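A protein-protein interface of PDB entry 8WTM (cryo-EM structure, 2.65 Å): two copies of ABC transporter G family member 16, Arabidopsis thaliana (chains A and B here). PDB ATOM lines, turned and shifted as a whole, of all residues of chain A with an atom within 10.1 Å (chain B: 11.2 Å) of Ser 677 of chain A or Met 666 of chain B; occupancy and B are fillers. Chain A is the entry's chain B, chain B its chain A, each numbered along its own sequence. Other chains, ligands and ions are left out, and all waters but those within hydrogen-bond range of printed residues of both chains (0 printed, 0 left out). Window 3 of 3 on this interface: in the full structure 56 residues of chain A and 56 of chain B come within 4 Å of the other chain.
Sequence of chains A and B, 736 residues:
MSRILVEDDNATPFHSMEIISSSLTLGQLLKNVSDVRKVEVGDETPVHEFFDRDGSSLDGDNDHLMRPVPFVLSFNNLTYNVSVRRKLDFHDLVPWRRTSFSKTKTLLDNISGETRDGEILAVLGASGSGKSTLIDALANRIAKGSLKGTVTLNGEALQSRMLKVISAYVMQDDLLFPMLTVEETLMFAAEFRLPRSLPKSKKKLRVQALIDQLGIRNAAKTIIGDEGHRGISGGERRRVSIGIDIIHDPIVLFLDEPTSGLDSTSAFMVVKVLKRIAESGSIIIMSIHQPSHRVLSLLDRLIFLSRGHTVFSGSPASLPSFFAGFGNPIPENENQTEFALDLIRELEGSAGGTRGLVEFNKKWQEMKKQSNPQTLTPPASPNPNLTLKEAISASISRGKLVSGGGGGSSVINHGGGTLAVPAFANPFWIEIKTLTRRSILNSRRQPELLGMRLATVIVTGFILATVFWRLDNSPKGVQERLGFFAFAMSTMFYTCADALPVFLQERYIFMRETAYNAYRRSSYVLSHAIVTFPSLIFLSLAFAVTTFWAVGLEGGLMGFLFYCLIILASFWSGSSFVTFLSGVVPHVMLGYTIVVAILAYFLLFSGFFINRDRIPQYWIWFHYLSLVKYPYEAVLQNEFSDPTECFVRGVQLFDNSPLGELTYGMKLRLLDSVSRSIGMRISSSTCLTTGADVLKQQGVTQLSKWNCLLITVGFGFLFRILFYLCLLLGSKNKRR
Leu 670 of chain A touches Val 674 of chain B (CD2 to CG1, 3.6 Å).
Leu 670 of chain A touches Ser 677 of chain B.
CG1 of Val 674 of chain A touches CD2 of Leu 659 of chain B, at 3.5 Å.
CD2 of Leu 670 of chain B touches CG1 of Val 674 of chain A, 3.6 Å away.
Met 666 of chain B touches Ser 677 of chain A.
OG of Ser 677 of chain A touches CD2 of Leu 670 of chain B, at 3.6 Å.
Ile 678 of chain A touches Leu 659 of chain B.
The backbone NH (N) of Met 666 of chain B sits at hydrogen-bond distance from the side-chain hydroxyl (OG1) of Thr 663 of chain B (3.2 Å).
The backbone carbonyl oxygen (O) of Leu 670 of chain B is in hydrogen-bond range of the side-chain hydroxyl (OG) of Ser 673 of chain B, at 2.9 Å.
The backbone carbonyl oxygen (O) of Leu 670 of chain A is in hydrogen-bond range of the side-chain hydroxyl (OG) of Ser 673 of chain A, 2.9 Å away.
Met 666 of chain B touches one residue of chain A.
Printed residues of chain A within 4 Å of Leu 659 of chain B: Val 674 and Ile 678.
Of the printed residues of chain A, Ser 677 of chain B touches Leu 670.
Of the printed residues of chain B, Leu 670 of chain A touches Val 674 and Ser 677.
Of the printed residues of chain A, Leu 670 of chain B touches Val 674 and Ser 677.
Arg 676 of chain A touches none of the printed residues of chain B.
Phe 654 of chain B touches none of the printed residues of chain A.
The nearest residue of chain A that does not touch Met 666 of chain B is Ile 678 of chain A (4.6 Å).
The nearest printed residue of chain A that does not touch Leu 670 of chain B is Ile 678 of chain A (4.02 Å).
Leu 670 of chain A touches Val 674 of chain B, and with the chains exchanged Val 674 of chain A touches Leu 670 of chain B.
Leu 670 of chain A touches Ser 677 of chain B, and with the chains exchanged Ser 677 of chain A touches Leu 670 of chain B.
8 positions are printed for both chains.
Of the 13 printed residues of chain A, 4 touch a printed residue of chain B.
Printed residues of chain A that touch a printed residue of chain B: Leu 670, Val 674, Ser 677 and Ile 678.
Hydrophobic or aromatic side chains of chain A that line the printed part of chain B: Leu 670, Val 674 and Ile 678.
Among the printed residues, 7 pairs touch across the chains.
Among the printed residues, no Asp or Glu carboxylate lies within 4 Å of a Lys or Arg side-chain nitrogen of the other chain.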
ATOM      1  N   LEU A 670      -9.612   4.866   8.208  1.00  0.00           N
ATOM      2  CA  LEU A 670     -10.646   3.890   8.535  1.00  0.00           C
ATOM      3  C   LEU A 670     -10.857   3.776  10.038  1.00  0.00           C
ATOM      4  O   LEU A 670     -11.933   3.360  10.477  1.00  0.00           O
ATOM      5  CB  LEU A 670     -10.301   2.518   7.958  1.00  0.00           C
ATOM      6  CG  LEU A 670     -10.397   2.360   6.446  1.00  0.00           C
ATOM      7  CD1 LEU A 670      -9.936   0.974   6.028  1.00  0.00           C
ATOM      8  CD2 LEU A 670     -11.827   2.604   6.013  1.00  0.00           C
ATOM      9  N   LEU A 671      -9.854   4.139  10.838  1.00  0.00           N
ATOM     10  CA  LEU A 671      -9.970   4.006  12.287  1.00  0.00           C
ATOM     11  C   LEU A 671     -10.805   5.122  12.905  1.00  0.00           C
ATOM     12  O   LEU A 671     -11.755   4.843  13.643  1.00  0.00           O
ATOM     13  CB  LEU A 671      -8.581   3.977  12.922  1.00  0.00           C
ATOM     14  CG  LEU A 671      -7.854   2.637  12.865  1.00  0.00           C
ATOM     15  CD1 LEU A 671      -6.517   2.753  13.551  1.00  0.00           C
ATOM     16  CD2 LEU A 671      -8.699   1.563  13.515  1.00  0.00           C
ATOM     17  N   ASP A 672     -10.473   6.385  12.624  1.00  0.00           N
ATOM     18  CA  ASP A 672     -11.180   7.489  13.262  1.00  0.00           C
ATOM     19  C   ASP A 672     -12.577   7.711  12.694  1.00  0.00           C
ATOM     20  O   ASP A 672     -13.385   8.397  13.328  1.00  0.00           O
ATOM     21  CB  ASP A 672     -10.356   8.781  13.171  1.00  0.00           C
ATOM     22  CG  ASP A 672     -10.015   9.170  11.745  1.00  0.00           C
ATOM     23  OD1 ASP A 672     -10.302   8.392  10.813  1.00  0.00           O
ATOM     24  OD2 ASP A 672      -9.463  10.272  11.550  1.00  0.00           O
ATOM     25  N   SER A 673     -12.873   7.153  11.517  1.00  0.00           N
ATOM     26  CA  SER A 673     -14.231   7.190  10.986  1.00  0.00           C
ATOM     27  C   SER A 673     -15.182   6.307  11.783  1.00  0.00           C
ATOM     28  O   SER A 673     -16.397   6.521  11.733  1.00  0.00           O
ATOM     29  CB  SER A 673     -14.232   6.768   9.520  1.00  0.00           C
ATOM     30  OG  SER A 673     -13.485   5.581   9.336  1.00  0.00           O
ATOM     31  N   VAL A 674     -14.653   5.321  12.511  1.00  0.00           N
ATOM     32  CA  VAL A 674     -15.444   4.579  13.486  1.00  0.00           C
ATOM     33  C   VAL A 674     -15.585   5.357  14.788  1.00  0.00           C
ATOM     34  O   VAL A 674     -16.601   5.212  15.485  1.00  0.00           O
ATOM     35  CB  VAL A 674     -14.803   3.191  13.706  1.00  0.00           C
ATOM     36  CG1 VAL A 674     -15.704   2.275  14.517  1.00  0.00           C
ATOM     37  CG2 VAL A 674     -14.483   2.546  12.372  1.00  0.00           C
ATOM     38  N   SER A 675     -14.631   6.234  15.105  1.00  0.00           N
ATOM     39  CA  SER A 675     -14.687   7.002  16.342  1.00  0.00           C
ATOM     40  C   SER A 675     -15.727   8.113  16.304  1.00  0.00           C
ATOM     41  O   SER A 675     -16.107   8.614  17.368  1.00  0.00           O
ATOM     42  CB  SER A 675     -13.315   7.601  16.658  1.00  0.00           C
ATOM     43  OG  SER A 675     -13.013   8.667  15.776  1.00  0.00           O
ATOM     44  N   ARG A 676     -16.178   8.523  15.114  1.00  0.00           N
ATOM     45  CA  ARG A 676     -17.246   9.515  15.035  1.00  0.00           C
ATOM     46  C   ARG A 676     -18.567   8.948  15.530  1.00  0.00           C
ATOM     47  O   ARG A 676     -19.380   9.679  16.108  1.00  0.00           O
ATOM     48  CB  ARG A 676     -17.423  10.003  13.598  1.00  0.00           C
ATOM     49  CG  ARG A 676     -16.154  10.112  12.782  1.00  0.00           C
ATOM     50  CD  ARG A 676     -15.449  11.436  12.997  1.00  0.00           C
ATOM     51  NE  ARG A 676     -14.603  11.762  11.854  1.00  0.00           N
ATOM     52  CZ  ARG A 676     -13.276  11.713  11.874  1.00  0.00           C
ATOM     53  NH1 ARG A 676     -12.647  11.354  12.983  1.00  0.00           N
ATOM     54  NH2 ARG A 676     -12.581  12.020  10.789  1.00  0.00           N
ATOM     55  N   SER A 677     -18.788   7.651  15.319  1.00  0.00           N
ATOM     56  CA  SER A 677     -20.061   7.026  15.653  1.00  0.00           C
ATOM     57  C   SER A 677     -20.205   6.825  17.157  1.00  0.00           C
ATOM     58  O   SER A 677     -21.129   7.360  17.780  1.00  0.00           O
ATOM     59  CB  SER A 677     -20.183   5.691  14.919  1.00  0.00           C
ATOM     60  OG  SER A 677     -19.729   5.808  13.581  1.00  0.00           O
ATOM     61  N   ILE A 678     -19.292   6.063  17.753  1.00  0.00           N
ATOM     62  CA  ILE A 678     -19.441   5.658  19.148  1.00  0.00           C
ATOM     63  C   ILE A 678     -19.033   6.784  20.088  1.00  0.00           C
ATOM     64  O   ILE A 678     -19.771   7.143  21.012  1.00  0.00           O
ATOM     65  CB  ILE A 678     -18.624   4.379  19.421  1.00  0.00           C
ATOM     66  CG1 ILE A 678     -19.067   3.245  18.496  1.00  0.00           C
ATOM     67  CG2 ILE A 678     -18.775   3.947  20.868  1.00  0.00           C
ATOM     68  CD1 ILE A 678     -18.074   2.910  17.406  1.00  0.00           C
ATOM     69  N   GLY A 679     -17.849   7.359  19.865  1.00  0.00           N
ATOM     70  CA  GLY A 679     -17.235   8.301  20.775  1.00  0.00           C
ATOM     71  C   GLY A 679     -15.942   7.787  21.377  1.00  0.00           C
ATOM     72  O   GLY A 679     -15.095   8.592  21.784  1.00  0.00           O
ATOM     73  N   MET A 680     -15.783   6.468  21.450  1.00  0.00           N
ATOM     74  CA  MET A 680     -14.503   5.880  21.821  1.00  0.00           C
ATOM     75  C   MET A 680     -13.488   6.109  20.710  1.00  0.00           C
ATOM     76  O   MET A 680     -13.767   5.855  19.535  1.00  0.00           O
ATOM     77  CB  MET A 680     -14.664   4.385  22.093  1.00  0.00           C
ATOM     78  CG  MET A 680     -13.380   3.681  22.514  1.00  0.00           C
ATOM     79  SD  MET A 680     -12.733   4.195  24.118  1.00  0.00           S
ATOM     80  CE  MET A 680     -13.886   3.373  25.217  1.00  0.00           C
ATOM     81  N   ARG A 681     -12.312   6.594  21.085  1.00  0.00           N
ATOM     82  CA  ARG A 681     -11.254   6.901  20.134  1.00  0.00           C
ATOM     83  C   ARG A 681     -10.326   5.696  20.045  1.00  0.00           C
ATOM     84  O   ARG A 681      -9.712   5.305  21.042  1.00  0.00           O
ATOM     85  CB  ARG A 681     -10.492   8.157  20.559  1.00  0.00           C
ATOM     86  CG  ARG A 681      -9.608   8.780  19.478  1.00  0.00           C
ATOM     87  CD  ARG A 681      -8.155   8.330  19.556  1.00  0.00           C
ATOM     88  NE  ARG A 681      -7.312   9.007  18.572  1.00  0.00           N
ATOM     89  CZ  ARG A 681      -7.183   8.633  17.302  1.00  0.00           C
ATOM     90  NH1 ARG A 681      -7.854   7.589  16.837  1.00  0.00           N
ATOM     91  NH2 ARG A 681      -6.390   9.315  16.490  1.00  0.00           N
ATOM     92  N   ILE A 682     -10.230   5.115  18.856  1.00  0.00           N
ATOM     93  CA  ILE A 682      -9.345   3.986  18.599  1.00  0.00           C
ATOM     94  C   ILE A 682      -8.126   4.536  17.871  1.00  0.00           C
ATOM     95  O   ILE A 682      -8.215   4.960  16.717  1.00  0.00           O
ATOM     96  CB  ILE A 682     -10.040   2.877  17.794  1.00  0.00           C
ATOM     97  CG1 ILE A 682     -11.172   2.227  18.600  1.00  0.00           C
ATOM     98  CG2 ILE A 682      -9.043   1.811  17.376  1.00  0.00           C
ATOM     99  CD1 ILE A 682     -12.556   2.798  18.349  1.00  0.00           C
ATOM    100  N   GLY B 650     -22.126  -8.551   5.903  1.00  0.00           N
ATOM    101  CA  GLY B 650     -22.522  -7.208   6.288  1.00  0.00           C
ATOM    102  C   GLY B 650     -22.027  -6.707   7.629  1.00  0.00           C
ATOM    103  O   GLY B 650     -20.861  -6.336   7.781  1.00  0.00           O
ATOM    104  N   VAL B 651     -22.935  -6.679   8.608  1.00  0.00           N
ATOM    105  CA  VAL B 651     -22.608  -6.236   9.959  1.00  0.00           C
ATOM    106  C   VAL B 651     -21.809  -7.255  10.757  1.00  0.00           C
ATOM    107  O   VAL B 651     -21.408  -6.955  11.885  1.00  0.00           O
ATOM    108  CB  VAL B 651     -23.890  -5.893  10.743  1.00  0.00           C
ATOM    109  CG1 VAL B 651     -24.740  -4.912   9.965  1.00  0.00           C
ATOM    110  CG2 VAL B 651     -24.680  -7.153  11.048  1.00  0.00           C
ATOM    111  N   GLN B 652     -21.553  -8.445  10.208  1.00  0.00           N
ATOM    112  CA  GLN B 652     -20.777  -9.471  10.896  1.00  0.00           C
ATOM    113  C   GLN B 652     -19.274  -9.240  10.817  1.00  0.00           C
ATOM    114  O   GLN B 652     -18.509 -10.117  11.224  1.00  0.00           O
ATOM    115  CB  GLN B 652     -21.111 -10.853  10.332  1.00  0.00           C
ATOM    116  CG  GLN B 652     -22.345 -11.482  10.933  1.00  0.00           C
ATOM    117  CD  GLN B 652     -22.961 -12.520  10.024  1.00  0.00           C
ATOM    118  OE1 GLN B 652     -22.654 -12.582   8.837  1.00  0.00           O
ATOM    119  NE2 GLN B 652     -23.844 -13.341  10.578  1.00  0.00           N
ATOM    120  N   PHE B 654     -17.733  -7.135  12.652  1.00  0.00           N
ATOM    121  CA  PHE B 654     -17.310  -6.679  13.970  1.00  0.00           C
ATOM    122  C   PHE B 654     -17.755  -7.633  15.074  1.00  0.00           C
ATOM    123  O   PHE B 654     -18.196  -7.206  16.141  1.00  0.00           O
ATOM    124  CB  PHE B 654     -17.850  -5.277  14.252  1.00  0.00           C
ATOM    125  CG  PHE B 654     -17.692  -4.314  13.112  1.00  0.00           C
ATOM    126  CD1 PHE B 654     -16.447  -3.807  12.781  1.00  0.00           C
ATOM    127  CD2 PHE B 654     -18.794  -3.901  12.384  1.00  0.00           C
ATOM    128  CE1 PHE B 654     -16.303  -2.908  11.736  1.00  0.00           C
ATOM    129  CE2 PHE B 654     -18.659  -3.006  11.337  1.00  0.00           C
ATOM    130  CZ  PHE B 654     -17.412  -2.511  11.012  1.00  0.00           C
ATOM    131  N   PRO B 658     -13.333  -5.907  19.878  1.00  0.00           N
ATOM    132  CA  PRO B 658     -13.976  -5.021  20.866  1.00  0.00           C
ATOM    133  C   PRO B 658     -14.866  -3.963  20.247  1.00  0.00           C
ATOM    134  O   PRO B 658     -15.858  -3.557  20.866  1.00  0.00           O
ATOM    135  CB  PRO B 658     -12.784  -4.395  21.598  1.00  0.00           C
ATOM    136  CG  PRO B 658     -11.720  -5.416  21.478  1.00  0.00           C
ATOM    137  CD  PRO B 658     -11.881  -5.998  20.105  1.00  0.00           C
ATOM    138  N   LEU B 659     -14.540  -3.498  19.049  1.00  0.00           N
ATOM    139  CA  LEU B 659     -15.515  -2.776  18.248  1.00  0.00           C
ATOM    140  C   LEU B 659     -16.576  -3.762  17.778  1.00  0.00           C
ATOM    141  O   LEU B 659     -16.255  -4.757  17.121  1.00  0.00           O
ATOM    142  CB  LEU B 659     -14.830  -2.108  17.059  1.00  0.00           C
ATOM    143  CG  LEU B 659     -15.702  -1.616  15.901  1.00  0.00           C
ATOM    144  CD1 LEU B 659     -16.729  -0.580  16.356  1.00  0.00           C
ATOM    145  CD2 LEU B 659     -14.839  -1.066  14.775  1.00  0.00           C
ATOM    146  N   GLY B 660     -17.832  -3.504  18.129  1.00  0.00           N
ATOM    147  CA  GLY B 660     -18.906  -4.351  17.647  1.00  0.00           C
ATOM    148  C   GLY B 660     -19.680  -5.093  18.713  1.00  0.00           C
ATOM    149  O   GLY B 660     -20.152  -6.211  18.482  1.00  0.00           O
ATOM    150  N   GLU B 661     -19.813  -4.488  19.888  1.00  0.00           N
ATOM    151  CA  GLU B 661     -20.725  -4.978  20.919  1.00  0.00           C
ATOM    152  C   GLU B 661     -21.986  -4.138  20.975  1.00  0.00           C
ATOM    153  O   GLU B 661     -22.555  -3.906  22.044  1.00  0.00           O
ATOM    154  CB  GLU B 661     -20.022  -4.995  22.273  1.00  0.00           C
ATOM    155  CG  GLU B 661     -18.906  -6.016  22.379  1.00  0.00           C
ATOM    156  CD  GLU B 661     -19.419  -7.442  22.364  1.00  0.00           C
ATOM    157  OE1 GLU B 661     -20.535  -7.680  22.876  1.00  0.00           O
ATOM    158  OE2 GLU B 661     -18.710  -8.326  21.836  1.00  0.00           O
ATOM    159  N   LEU B 662     -22.436  -3.671  19.820  1.00  0.00           N
ATOM    160  CA  LEU B 662     -23.442  -2.633  19.711  1.00  0.00           C
ATOM    161  C   LEU B 662     -24.728  -3.209  19.118  1.00  0.00           C
ATOM    162  O   LEU B 662     -24.848  -4.417  18.881  1.00  0.00           O
ATOM    163  CB  LEU B 662     -22.893  -1.467  18.882  1.00  0.00           C
ATOM    164  CG  LEU B 662     -22.016  -0.406  19.571  1.00  0.00           C
ATOM    165  CD1 LEU B 662     -22.779   0.268  20.709  1.00  0.00           C
ATOM    166  CD2 LEU B 662     -20.635  -0.901  20.030  1.00  0.00           C
ATOM    167  N   THR B 663     -25.694  -2.332  18.867  1.00  0.00           N
ATOM    168  CA  THR B 663     -26.999  -2.731  18.370  1.00  0.00           C
ATOM    169  C   THR B 663     -26.954  -2.899  16.854  1.00  0.00           C
ATOM    170  O   THR B 663     -25.930  -2.669  16.204  1.00  0.00           O
ATOM    171  CB  THR B 663     -28.061  -1.706  18.770  1.00  0.00           C
ATOM    172  OG1 THR B 663     -28.039  -0.610  17.848  1.00  0.00           O
ATOM    173  CG2 THR B 663     -27.795  -1.182  20.173  1.00  0.00           C
ATOM    174  N   TYR B 664     -28.091  -3.308  16.286  1.00  0.00           N
ATOM    175  CA  TYR B 664     -28.173  -3.489  14.842  1.00  0.00           C
ATOM    176  C   TYR B 664     -28.152  -2.155  14.110  1.00  0.00           C
ATOM    177  O   TYR B 664     -27.522  -2.044  13.054  1.00  0.00           O
ATOM    178  CB  TYR B 664     -29.438  -4.276  14.485  1.00  0.00           C
ATOM    179  CG  TYR B 664     -29.432  -4.901  13.103  1.00  0.00           C
ATOM    180  CD1 TYR B 664     -29.106  -6.242  12.931  1.00  0.00           C
ATOM    181  CD2 TYR B 664     -29.787  -4.162  11.974  1.00  0.00           C
ATOM    182  CE1 TYR B 664     -29.107  -6.821  11.676  1.00  0.00           C
ATOM    183  CE2 TYR B 664     -29.790  -4.734  10.717  1.00  0.00           C
ATOM    184  CZ  TYR B 664     -29.450  -6.063  10.575  1.00  0.00           C
ATOM    185  OH  TYR B 664     -29.452  -6.638   9.327  1.00  0.00           O
ATOM    186  N   GLY B 665     -28.813  -1.135  14.660  1.00  0.00           N
ATOM    187  CA  GLY B 665     -28.861   0.153  13.986  1.00  0.00           C
ATOM    188  C   GLY B 665     -27.541   0.893  14.065  1.00  0.00           C
ATOM    189  O   GLY B 665     -27.188   1.662  13.166  1.00  0.00           O
ATOM    190  N   MET B 666     -26.794   0.665  15.142  1.00  0.00           N
ATOM    191  CA  MET B 666     -25.518   1.329  15.357  1.00  0.00           C
ATOM    192  C   MET B 666     -24.447   0.854  14.385  1.00  0.00           C
ATOM    193  O   MET B 666     -23.644   1.670  13.919  1.00  0.00           O
ATOM    194  CB  MET B 666     -25.054   1.082  16.798  1.00  0.00           C
ATOM    195  CG  MET B 666     -23.770   1.778  17.212  1.00  0.00           C
ATOM    196  SD  MET B 666     -23.961   3.551  17.488  1.00  0.00           S
ATOM    197  CE  MET B 666     -23.177   4.216  16.029  1.00  0.00           C
ATOM    198  N   LYS B 667     -24.443  -0.437  14.038  1.00  0.00           N
ATOM    199  CA  LYS B 667     -23.445  -0.963  13.111  1.00  0.00           C
ATOM    200  C   LYS B 667     -23.804  -0.677  11.657  1.00  0.00           C
ATOM    201  O   LYS B 667     -22.937  -0.779  10.782  1.00  0.00           O
ATOM    202  CB  LYS B 667     -23.263  -2.465  13.330  1.00  0.00           C
ATOM    203  CG  LYS B 667     -22.573  -2.809  14.635  1.00  0.00           C
ATOM    204  CD  LYS B 667     -22.310  -4.297  14.772  1.00  0.00           C
ATOM    205  CE  LYS B 667     -23.583  -5.054  15.109  1.00  0.00           C
ATOM    206  NZ  LYS B 667     -23.298  -6.477  15.428  1.00  0.00           N
ATOM    207  N   LEU B 668     -25.067  -0.338  11.373  1.00  0.00           N
ATOM    208  CA  LEU B 668     -25.441  -0.003  10.001  1.00  0.00           C
ATOM    209  C   LEU B 668     -24.820   1.312   9.552  1.00  0.00           C
ATOM    210  O   LEU B 668     -24.483   1.460   8.373  1.00  0.00           O
ATOM    211  CB  LEU B 668     -26.960   0.044   9.847  1.00  0.00           C
ATOM    212  CG  LEU B 668     -27.682  -1.303   9.853  1.00  0.00           C
ATOM    213  CD1 LEU B 668     -29.188  -1.111   9.813  1.00  0.00           C
ATOM    214  CD2 LEU B 668     -27.213  -2.159   8.690  1.00  0.00           C
ATOM    215  N   ARG B 669     -24.656   2.270  10.463  1.00  0.00           N
ATOM    216  CA  ARG B 669     -23.862   3.441  10.124  1.00  0.00           C
ATOM    217  C   ARG B 669     -22.369   3.213  10.322  1.00  0.00           C
ATOM    218  O   ARG B 669     -21.570   4.048   9.890  1.00  0.00           O
ATOM    219  CB  ARG B 669     -24.336   4.673  10.910  1.00  0.00           C
ATOM    220  CG  ARG B 669     -24.050   4.678  12.394  1.00  0.00           C
ATOM    221  CD  ARG B 669     -25.087   5.530  13.116  1.00  0.00           C
ATOM    222  NE  ARG B 669     -26.407   4.905  13.126  1.00  0.00           N
ATOM    223  CZ  ARG B 669     -27.312   5.095  14.081  1.00  0.00           C
ATOM    224  NH1 ARG B 669     -28.489   4.487  14.017  1.00  0.00           N
ATOM    225  NH2 ARG B 669     -27.037   5.894  15.102  1.00  0.00           N
ATOM    226  N   LEU B 670     -21.970   2.100  10.944  1.00  0.00           N
ATOM    227  CA  LEU B 670     -20.565   1.710  10.910  1.00  0.00           C
ATOM    228  C   LEU B 670     -20.170   1.149   9.552  1.00  0.00           C
ATOM    229  O   LEU B 670     -18.988   1.177   9.195  1.00  0.00           O
ATOM    230  CB  LEU B 670     -20.257   0.685  12.000  1.00  0.00           C
ATOM    231  CG  LEU B 670     -20.255   1.183  13.439  1.00  0.00           C
ATOM    232  CD1 LEU B 670     -20.025   0.029  14.400  1.00  0.00           C
ATOM    233  CD2 LEU B 670     -19.178   2.235  13.595  1.00  0.00           C
ATOM    234  N   LEU B 671     -21.133   0.641   8.782  1.00  0.00           N
ATOM    235  CA  LEU B 671     -20.818   0.041   7.490  1.00  0.00           C
ATOM    236  C   LEU B 671     -20.571   1.087   6.410  1.00  0.00           C
ATOM    237  O   LEU B 671     -19.535   1.047   5.740  1.00  0.00           O
ATOM    238  CB  LEU B 671     -21.943  -0.900   7.062  1.00  0.00           C
ATOM    239  CG  LEU B 671     -21.928  -2.285   7.702  1.00  0.00           C
ATOM    240  CD1 LEU B 671     -23.074  -3.106   7.166  1.00  0.00           C
ATOM    241  CD2 LEU B 671     -20.605  -2.967   7.426  1.00  0.00           C
ATOM    242  N   ASP B 672     -21.503   2.025   6.220  1.00  0.00           N
ATOM    243  CA  ASP B 672     -21.358   2.994   5.139  1.00  0.00           C
ATOM    244  C   ASP B 672     -20.313   4.064   5.431  1.00  0.00           C
ATOM    245  O   ASP B 672     -19.879   4.754   4.503  1.00  0.00           O
ATOM    246  CB  ASP B 672     -22.711   3.644   4.815  1.00  0.00           C
ATOM    247  CG  ASP B 672     -23.344   4.329   6.012  1.00  0.00           C
ATOM    248  OD1 ASP B 672     -22.814   4.212   7.134  1.00  0.00           O
ATOM    249  OD2 ASP B 672     -24.379   5.002   5.827  1.00  0.00           O
ATOM    250  N   SER B 673     -19.908   4.220   6.694  1.00  0.00           N
ATOM    251  CA  SER B 673     -18.803   5.111   7.026  1.00  0.00           C
ATOM    252  C   SER B 673     -17.465   4.574   6.534  1.00  0.00           C
ATOM    253  O   SER B 673     -16.519   5.352   6.372  1.00  0.00           O
ATOM    254  CB  SER B 673     -18.749   5.339   8.534  1.00  0.00           C
ATOM    255  OG  SER B 673     -18.840   4.113   9.234  1.00  0.00           O
ATOM    256  N   VAL B 674     -17.369   3.263   6.296  1.00  0.00           N
ATOM    257  CA  VAL B 674     -16.221   2.693   5.602  1.00  0.00           C
ATOM    258  C   VAL B 674     -16.342   2.876   4.094  1.00  0.00           C
ATOM    259  O   VAL B 674     -15.316   2.990   3.404  1.00  0.00           O
ATOM    260  CB  VAL B 674     -16.080   1.206   5.996  1.00  0.00           C
ATOM    261  CG1 VAL B 674     -14.769   0.615   5.509  1.00  0.00           C
ATOM    262  CG2 VAL B 674     -16.183   1.052   7.500  1.00  0.00           C
ATOM    263  N   SER B 675     -17.563   2.981   3.568  1.00  0.00           N
ATOM    264  CA  SER B 675     -17.758   3.139   2.133  1.00  0.00           C
ATOM    265  C   SER B 675     -17.400   4.532   1.635  1.00  0.00           C
ATOM    266  O   SER B 675     -17.203   4.706   0.427  1.00  0.00           O
ATOM    267  CB  SER B 675     -19.207   2.823   1.756  1.00  0.00           C
ATOM    268  OG  SER B 675     -20.079   3.851   2.190  1.00  0.00           O
ATOM    269  N   ARG B 676     -17.331   5.528   2.525  1.00  0.00           N
ATOM    270  CA  ARG B 676     -16.895   6.857   2.108  1.00  0.00           C
ATOM    271  C   ARG B 676     -15.422   6.865   1.733  1.00  0.00           C
ATOM    272  O   ARG B 676     -15.011   7.614   0.838  1.00  0.00           O
ATOM    273  CB  ARG B 676     -17.129   7.876   3.223  1.00  0.00           C
ATOM    274  CG  ARG B 676     -18.367   7.656   4.063  1.00  0.00           C
ATOM    275  CD  ARG B 676     -19.600   8.273   3.433  1.00  0.00           C
ATOM    276  NE  ARG B 676     -20.612   8.554   4.446  1.00  0.00           N
ATOM    277  CZ  ARG B 676     -21.737   7.863   4.583  1.00  0.00           C
ATOM    278  NH1 ARG B 676     -21.993   6.852   3.767  1.00  0.00           N
ATOM    279  NH2 ARG B 676     -22.602   8.181   5.535  1.00  0.00           N
ATOM    280  N   SER B 677     -14.622   6.034   2.399  1.00  0.00           N
ATOM    281  CA  SER B 677     -13.178   6.033   2.198  1.00  0.00           C
ATOM    282  C   SER B 677     -12.799   5.372   0.878  1.00  0.00           C
ATOM    283  O   SER B 677     -12.193   6.002   0.006  1.00  0.00           O
ATOM    284  CB  SER B 677     -12.500   5.323   3.369  1.00  0.00           C
ATOM    285  OG  SER B 677     -13.090   5.706   4.601  1.00  0.00           O
ATOM    286  N   SER B 684     -25.854  -4.217   4.004  1.00  0.00           N
ATOM    287  CA  SER B 684     -26.156  -5.091   5.130  1.00  0.00           C
ATOM    288  C   SER B 684     -25.981  -6.558   4.769  1.00  0.00           C
ATOM    289  O   SER B 684     -25.780  -7.385   5.664  1.00  0.00           O
ATOM    290  CB  SER B 684     -27.581  -4.840   5.625  1.00  0.00           C
ATOM    291  OG  SER B 684     -27.917  -5.720   6.683  1.00  0.00           O
